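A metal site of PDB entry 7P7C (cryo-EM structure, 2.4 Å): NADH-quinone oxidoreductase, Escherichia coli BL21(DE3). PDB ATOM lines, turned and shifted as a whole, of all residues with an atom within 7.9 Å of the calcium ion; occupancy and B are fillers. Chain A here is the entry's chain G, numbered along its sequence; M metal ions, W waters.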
ATOM      1  N   ALA A 610      13.162  -5.142 -15.559  1.00  0.00           N
ATOM      2  CA  ALA A 610      14.428  -4.454 -15.547  1.00  0.00           C
ATOM      3  C   ALA A 610      15.553  -5.431 -15.823  1.00  0.00           C
ATOM      4  O   ALA A 610      15.489  -6.607 -15.447  1.00  0.00           O
ATOM      5  CB  ALA A 610      14.652  -3.761 -14.206  1.00  0.00           C
ATOM      6  N   GLU A 614      19.144  -2.038 -13.983  1.00  0.00           N
ATOM      7  CA  GLU A 614      17.993  -1.327 -13.452  1.00  0.00           C
ATOM      8  C   GLU A 614      17.262  -2.121 -12.365  1.00  0.00           C
ATOM      9  O   GLU A 614      16.125  -1.793 -12.030  1.00  0.00           O
ATOM     10  CB  GLU A 614      17.036  -0.964 -14.577  1.00  0.00           C
ATOM     11  CG  GLU A 614      17.725  -0.326 -15.774  1.00  0.00           C
ATOM     12  CD  GLU A 614      17.697  -1.199 -17.006  1.00  0.00           C
ATOM     13  OE1 GLU A 614      17.199  -2.332 -16.914  1.00  0.00           O
ATOM     14  OE2 GLU A 614      18.185  -0.764 -18.070  1.00  0.00           O
ATOM     15  N   SER A 615      17.897  -3.146 -11.802  1.00  0.00           N
ATOM     16  CA  SER A 615      17.249  -3.980 -10.812  1.00  0.00           C
ATOM     17  C   SER A 615      18.222  -4.344  -9.705  1.00  0.00           C
ATOM     18  O   SER A 615      19.442  -4.260  -9.860  1.00  0.00           O
ATOM     19  CB  SER A 615      16.681  -5.264 -11.438  1.00  0.00           C
ATOM     20  OG  SER A 615      17.717  -6.099 -11.905  1.00  0.00           O
ATOM     21  N   ASP A 616      17.657  -4.769  -8.573  1.00  0.00           N
ATOM     22  CA  ASP A 616      18.397  -5.355  -7.465  1.00  0.00           C
ATOM     23  C   ASP A 616      18.027  -6.831  -7.357  1.00  0.00           C
ATOM     24  O   ASP A 616      16.943  -7.234  -7.771  1.00  0.00           O
ATOM     25  CB  ASP A 616      18.080  -4.643  -6.149  1.00  0.00           C
ATOM     26  CG  ASP A 616      18.076  -3.132  -6.279  1.00  0.00           C
ATOM     27  OD1 ASP A 616      19.170  -2.531  -6.247  1.00  0.00           O
ATOM     28  OD2 ASP A 616      16.992  -2.555  -6.419  1.00  0.00           O
ATOM     29  N   GLY A 617      18.934  -7.621  -6.800  1.00  0.00           N
ATOM     30  CA  GLY A 617      18.616  -9.023  -6.621  1.00  0.00           C
ATOM     31  C   GLY A 617      19.788  -9.807  -6.089  1.00  0.00           C
ATOM     32  O   GLY A 617      20.836  -9.245  -5.777  1.00  0.00           O
ATOM     33  N   PHE A 630      23.035  -4.626  -7.250  1.00  0.00           N
ATOM     34  CA  PHE A 630      22.292  -3.424  -6.926  1.00  0.00           C
ATOM     35  C   PHE A 630      21.965  -2.664  -8.206  1.00  0.00           C
ATOM     36  O   PHE A 630      22.670  -2.773  -9.205  1.00  0.00           O
ATOM     37  CB  PHE A 630      23.084  -2.518  -5.978  1.00  0.00           C
ATOM     38  CG  PHE A 630      23.418  -3.154  -4.655  1.00  0.00           C
ATOM     39  CD1 PHE A 630      24.511  -3.982  -4.515  1.00  0.00           C
ATOM     40  CD2 PHE A 630      22.634  -2.920  -3.546  1.00  0.00           C
ATOM     41  CE1 PHE A 630      24.811  -4.570  -3.297  1.00  0.00           C
ATOM     42  CE2 PHE A 630      22.922  -3.495  -2.329  1.00  0.00           C
ATOM     43  CZ  PHE A 630      24.009  -4.314  -2.207  1.00  0.00           C
ATOM     44  N   GLN A 631      20.868  -1.914  -8.161  1.00  0.00           N
ATOM     45  CA  GLN A 631      20.459  -1.103  -9.301  1.00  0.00           C
ATOM     46  C   GLN A 631      21.460   0.026  -9.538  1.00  0.00           C
ATOM     47  O   GLN A 631      21.949   0.649  -8.600  1.00  0.00           O
ATOM     48  CB  GLN A 631      19.061  -0.536  -9.055  1.00  0.00           C
ATOM     49  CG  GLN A 631      18.537   0.361 -10.157  1.00  0.00           C
ATOM     50  CD  GLN A 631      17.048   0.616 -10.044  1.00  0.00           C
ATOM     51  OE1 GLN A 631      16.360   0.047  -9.203  1.00  0.00           O
ATOM     52  NE2 GLN A 631      16.536   1.486 -10.914  1.00  0.00           N
ATOM     53  N   VAL A 632      21.758   0.282 -10.807  1.00  0.00           N
ATOM     54  CA  VAL A 632      22.718   1.320 -11.165  1.00  0.00           C
ATOM     55  C   VAL A 632      22.039   2.677 -11.313  1.00  0.00           C
ATOM     56  O   VAL A 632      22.499   3.678 -10.749  1.00  0.00           O
ATOM     57  CB  VAL A 632      23.484   0.931 -12.449  1.00  0.00           C
ATOM     58  CG1 VAL A 632      24.678   1.839 -12.648  1.00  0.00           C
ATOM     59  CG2 VAL A 632      23.914  -0.498 -12.366  1.00  0.00           C
ATOM     60  N   TYR A 633      20.938   2.733 -12.061  1.00  0.00           N
ATOM     61  CA  TYR A 633      20.267   3.992 -12.302  1.00  0.00           C
ATOM     62  C   TYR A 633      18.764   3.759 -12.338  1.00  0.00           C
ATOM     63  O   TYR A 633      18.286   2.629 -12.479  1.00  0.00           O
ATOM     64  CB  TYR A 633      20.750   4.638 -13.604  1.00  0.00           C
ATOM     65  CG  TYR A 633      20.287   3.951 -14.862  1.00  0.00           C
ATOM     66  CD1 TYR A 633      20.931   2.810 -15.333  1.00  0.00           C
ATOM     67  CD2 TYR A 633      19.229   4.448 -15.604  1.00  0.00           C
ATOM     68  CE1 TYR A 633      20.512   2.176 -16.481  1.00  0.00           C
ATOM     69  CE2 TYR A 633      18.798   3.825 -16.753  1.00  0.00           C
ATOM     70  CZ  TYR A 633      19.441   2.687 -17.187  1.00  0.00           C
ATOM     71  OH  TYR A 633      19.017   2.079 -18.341  1.00  0.00           O
ATOM     72  N   ASP A 634      18.031   4.857 -12.219  1.00  0.00           N
ATOM     73  CA  ASP A 634      16.576   4.816 -12.379  1.00  0.00           C
ATOM     74  C   ASP A 634      16.232   5.049 -13.841  1.00  0.00           C
ATOM     75  O   ASP A 634      16.557   6.112 -14.380  1.00  0.00           O
ATOM     76  CB  ASP A 634      15.923   5.875 -11.509  1.00  0.00           C
ATOM     77  CG  ASP A 634      14.414   5.895 -11.652  1.00  0.00           C
ATOM     78  OD1 ASP A 634      13.787   4.838 -11.463  1.00  0.00           O
ATOM     79  OD2 ASP A 634      13.858   6.968 -11.976  1.00  0.00           O
ATOM     80  N   PRO A 635      15.593   4.081 -14.517  1.00  0.00           N
ATOM     81  CA  PRO A 635      15.275   4.269 -15.941  1.00  0.00           C
ATOM     82  C   PRO A 635      14.243   5.358 -16.205  1.00  0.00           C
ATOM     83  O   PRO A 635      14.175   5.865 -17.330  1.00  0.00           O
ATOM     84  CB  PRO A 635      14.746   2.893 -16.381  1.00  0.00           C
ATOM     85  CG  PRO A 635      14.927   1.989 -15.205  1.00  0.00           C
ATOM     86  CD  PRO A 635      15.070   2.822 -13.987  1.00  0.00           C
ATOM     87  N   LEU A 645      10.165  -2.135 -14.142  1.00  0.00           N
ATOM     88  CA  LEU A 645      10.287  -2.495 -12.749  1.00  0.00           C
ATOM     89  C   LEU A 645      11.098  -3.768 -12.574  1.00  0.00           C
ATOM     90  O   LEU A 645      11.365  -4.492 -13.534  1.00  0.00           O
ATOM     91  CB  LEU A 645       8.902  -2.664 -12.120  1.00  0.00           C
ATOM     92  CG  LEU A 645       8.065  -1.392 -12.001  1.00  0.00           C
ATOM     93  CD1 LEU A 645       6.664  -1.719 -11.540  1.00  0.00           C
ATOM     94  CD2 LEU A 645       8.733  -0.414 -11.054  1.00  0.00           C
ATOM     95  N   GLU A 646      11.500  -4.018 -11.333  1.00  0.00           N
ATOM     96  CA  GLU A 646      12.108  -5.299 -10.987  1.00  0.00           C
ATOM     97  C   GLU A 646      11.114  -6.428 -11.229  1.00  0.00           C
ATOM     98  O   GLU A 646       9.899  -6.249 -11.095  1.00  0.00           O
ATOM     99  CB  GLU A 646      12.531  -5.308  -9.522  1.00  0.00           C
ATOM    100  CG  GLU A 646      13.871  -4.664  -9.248  1.00  0.00           C
ATOM    101  CD  GLU A 646      13.755  -3.212  -8.850  1.00  0.00           C
ATOM    102  OE1 GLU A 646      12.744  -2.572  -9.193  1.00  0.00           O
ATOM    103  OE2 GLU A 646      14.678  -2.719  -8.176  1.00  0.00           O
ATOM    104  N   TRP A 648      10.747  -9.275  -9.564  1.00  0.00           N
ATOM    105  CA  TRP A 648      10.070  -9.680  -8.337  1.00  0.00           C
ATOM    106  C   TRP A 648       9.046  -8.649  -7.895  1.00  0.00           C
ATOM    107  O   TRP A 648       8.024  -8.999  -7.310  1.00  0.00           O
ATOM    108  CB  TRP A 648      11.069  -9.962  -7.215  1.00  0.00           C
ATOM    109  CG  TRP A 648      12.214  -9.013  -7.112  1.00  0.00           C
ATOM    110  CD1 TRP A 648      13.419  -9.116  -7.714  1.00  0.00           C
ATOM    111  CD2 TRP A 648      12.253  -7.800  -6.350  1.00  0.00           C
ATOM    112  NE1 TRP A 648      14.219  -8.058  -7.375  1.00  0.00           N
ATOM    113  CE2 TRP A 648      13.519  -7.227  -6.545  1.00  0.00           C
ATOM    114  CE3 TRP A 648      11.332  -7.140  -5.530  1.00  0.00           C
ATOM    115  CZ2 TRP A 648      13.903  -6.029  -5.942  1.00  0.00           C
ATOM    116  CZ3 TRP A 648      11.716  -5.950  -4.932  1.00  0.00           C
ATOM    117  CH2 TRP A 648      12.980  -5.412  -5.146  1.00  0.00           C
ATOM    118  N   ARG A 649       9.292  -7.368  -8.202  1.00  0.00           N
ATOM    119  CA  ARG A 649       8.296  -6.337  -7.926  1.00  0.00           C
ATOM    120  C   ARG A 649       7.043  -6.544  -8.771  1.00  0.00           C
ATOM    121  O   ARG A 649       5.926  -6.481  -8.245  1.00  0.00           O
ATOM    122  CB  ARG A 649       8.910  -4.959  -8.181  1.00  0.00           C
ATOM    123  CG  ARG A 649       8.004  -3.787  -7.856  1.00  0.00           C
ATOM    124  CD  ARG A 649       8.804  -2.525  -7.618  1.00  0.00           C
ATOM    125  NE  ARG A 649       9.136  -2.337  -6.214  1.00  0.00           N
ATOM    126  CZ  ARG A 649      10.347  -2.049  -5.764  1.00  0.00           C
ATOM    127  NH1 ARG A 649      11.374  -1.907  -6.575  1.00  0.00           N
ATOM    128  NH2 ARG A 649      10.533  -1.898  -4.452  1.00  0.00           N
ATOM    129  N   LEU A 668      12.468  -4.892  -1.211  1.00  0.00           N
ATOM    130  CA  LEU A 668      13.373  -5.998  -1.511  1.00  0.00           C
ATOM    131  C   LEU A 668      13.613  -6.898  -0.305  1.00  0.00           C
ATOM    132  O   LEU A 668      13.631  -8.123  -0.424  1.00  0.00           O
ATOM    133  CB  LEU A 668      14.708  -5.466  -2.051  1.00  0.00           C
ATOM    134  CG  LEU A 668      15.885  -6.448  -2.133  1.00  0.00           C
ATOM    135  CD1 LEU A 668      15.661  -7.524  -3.175  1.00  0.00           C
ATOM    136  CD2 LEU A 668      17.187  -5.714  -2.394  1.00  0.00           C
ATOM    137  N   ARG A 703      26.211   6.445  -4.979  1.00  0.00           N
ATOM    138  CA  ARG A 703      26.367   5.772  -6.255  1.00  0.00           C
ATOM    139  C   ARG A 703      27.209   6.546  -7.247  1.00  0.00           C
ATOM    140  O   ARG A 703      27.709   5.954  -8.211  1.00  0.00           O
ATOM    141  CB  ARG A 703      24.992   5.496  -6.883  1.00  0.00           C
ATOM    142  CG  ARG A 703      24.347   4.187  -6.483  1.00  0.00           C
ATOM    143  CD  ARG A 703      23.145   3.907  -7.363  1.00  0.00           C
ATOM    144  NE  ARG A 703      22.454   2.668  -7.027  1.00  0.00           N
ATOM    145  CZ  ARG A 703      21.453   2.580  -6.171  1.00  0.00           C
ATOM    146  NH1 ARG A 703      21.004   3.636  -5.514  1.00  0.00           N
ATOM    147  NH2 ARG A 703      20.874   1.402  -5.970  1.00  0.00           N
ATOM    148  N   GLN A 727      14.412   7.934  -5.484  1.00  0.00           N
ATOM    149  CA  GLN A 727      14.441   7.365  -4.142  1.00  0.00           C
ATOM    150  C   GLN A 727      14.695   5.870  -4.240  1.00  0.00           C
ATOM    151  O   GLN A 727      14.073   5.176  -5.043  1.00  0.00           O
ATOM    152  CB  GLN A 727      13.126   7.638  -3.408  1.00  0.00           C
ATOM    153  CG  GLN A 727      13.030   9.030  -2.799  1.00  0.00           C
ATOM    154  CD  GLN A 727      14.229   9.379  -1.940  1.00  0.00           C
ATOM    155  OE1 GLN A 727      14.839  10.428  -2.116  1.00  0.00           O
ATOM    156  NE2 GLN A 727      14.554   8.502  -0.988  1.00  0.00           N
ATOM    157  N   ASP A 728      15.626   5.383  -3.426  1.00  0.00           N
ATOM    158  CA  ASP A 728      15.968   3.973  -3.351  1.00  0.00           C
ATOM    159  C   ASP A 728      15.470   3.454  -2.009  1.00  0.00           C
ATOM    160  O   ASP A 728      16.157   3.538  -0.996  1.00  0.00           O
ATOM    161  CB  ASP A 728      17.469   3.750  -3.522  1.00  0.00           C
ATOM    162  CG  ASP A 728      17.816   2.304  -3.839  1.00  0.00           C
ATOM    163  OD1 ASP A 728      16.927   1.434  -3.768  1.00  0.00           O
ATOM    164  OD2 ASP A 728      18.990   2.037  -4.164  1.00  0.00           O
ATOM    165  N   ILE A 729      14.240   2.931  -2.011  1.00  0.00           N
ATOM    166  CA  ILE A 729      13.741   2.228  -0.832  1.00  0.00           C
ATOM    167  C   ILE A 729      14.178   0.767  -0.816  1.00  0.00           C
ATOM    168  O   ILE A 729      13.963   0.085   0.186  1.00  0.00           O
ATOM    169  CB  ILE A 729      12.206   2.290  -0.740  1.00  0.00           C
ATOM    170  CG1 ILE A 729      11.567   1.403  -1.812  1.00  0.00           C
ATOM    171  CG2 ILE A 729      11.727   3.722  -0.888  1.00  0.00           C
ATOM    172  CD1 ILE A 729      10.104   1.141  -1.591  1.00  0.00           C
ATOM    173  N   ASP A 730      14.787   0.298  -1.903  1.00  0.00           N
ATOM    174  CA  ASP A 730      15.146  -1.110  -1.999  1.00  0.00           C
ATOM    175  C   ASP A 730      16.433  -1.430  -1.258  1.00  0.00           C
ATOM    176  O   ASP A 730      16.518  -2.451  -0.570  1.00  0.00           O
ATOM    177  CB  ASP A 730      15.257  -1.501  -3.473  1.00  0.00           C
ATOM    178  CG  ASP A 730      13.911  -1.782  -4.114  1.00  0.00           C
ATOM    179  OD1 ASP A 730      13.057  -2.399  -3.447  1.00  0.00           O
ATOM    180  OD2 ASP A 730      13.710  -1.377  -5.276  1.00  0.00           O
ATOM    181  N   THR A 731      17.452  -0.592  -1.402  1.00  0.00           N
ATOM    182  CA  THR A 731      18.783  -0.895  -0.881  1.00  0.00           C
ATOM    183  C   THR A 731      19.323   0.270  -0.061  1.00  0.00           C
ATOM    184  O   THR A 731      18.672   1.307   0.104  1.00  0.00           O
ATOM    185  CB  THR A 731      19.770  -1.225  -2.014  1.00  0.00           C
ATOM    186  OG1 THR A 731      20.079  -0.039  -2.753  1.00  0.00           O
ATOM    187  CG2 THR A 731      19.218  -2.291  -2.953  1.00  0.00           C
ATOM    188  N   PHE A 735      20.756   7.220  -4.938  1.00  0.00           N
ATOM    189  CA  PHE A 735      20.976   7.584  -6.336  1.00  0.00           C
ATOM    190  C   PHE A 735      21.534   8.991  -6.473  1.00  0.00           C
ATOM    191  O   PHE A 735      21.018   9.800  -7.232  1.00  0.00           O
ATOM    192  CB  PHE A 735      19.680   7.446  -7.116  1.00  0.00           C
ATOM    193  CG  PHE A 735      19.277   6.035  -7.414  1.00  0.00           C
ATOM    194  CD1 PHE A 735      19.970   5.285  -8.351  1.00  0.00           C
ATOM    195  CD2 PHE A 735      18.207   5.455  -6.762  1.00  0.00           C
ATOM    196  CE1 PHE A 735      19.602   3.985  -8.624  1.00  0.00           C
ATOM    197  CE2 PHE A 735      17.827   4.158  -7.041  1.00  0.00           C
ATOM    198  CZ  PHE A 735      18.533   3.423  -7.962  1.00  0.00           C
HETATM  199 CA    CA M   1      15.435  -0.701  -6.987  1.00  0.00          CA
HETATM  200  O   HOH W   1      13.798   0.906  -8.120  1.00  0.00           O
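The backbone NH (N) of Gln 631 lies within hydrogen-bond range of the backbone carbonyl oxygen (O) of Ser 615 (3.2 Å).
The side-chain carboxylate (OE1) of Glu 646 lies within salt-bridge range of the guanidinium group (NH1) of Arg 649 (3.0 Å).
The side-chain carboxylate (OD1) of Asp 730 is in hydrogen-bond range of the backbone NH (N) of Leu 668.
O of Glu 614 sits close to NE2 of Gln 631 (3.5 Å).
The guanidinium group of Arg 703 sits at hydrogen-bond distance from the backbone carbonyl oxygen of Gln 631 (2.6 Å).
N of Asp 730 is in hydrogen-bond range of OD1 of Asp 728, 3.1 Å away.
O of Asp 616 lies within hydrogen-bond range of NE1 of Trp 648 (2.9 Å).
The backbone carbonyl oxygen of Tyr 633 lies within hydrogen-bond range of the side-chain amide nitrogen of Gln 631 (2.6 Å).
The nearest printed residue that does not touch the calcium ion is Asp 728 (4.1 Å).
The calcium ion is bound by OE2 of Glu 646 (2.5 Å).
OD2 of Asp 616 binds the calcium ion (2.5 Å).
OE1 of Gln 631 is bound to the calcium ion.
OD2 of Asp 730 binds the calcium ion.
Water W1 is bound to the calcium ion (2.6 Å).
The calcium ion has five donor atoms within binding distance.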
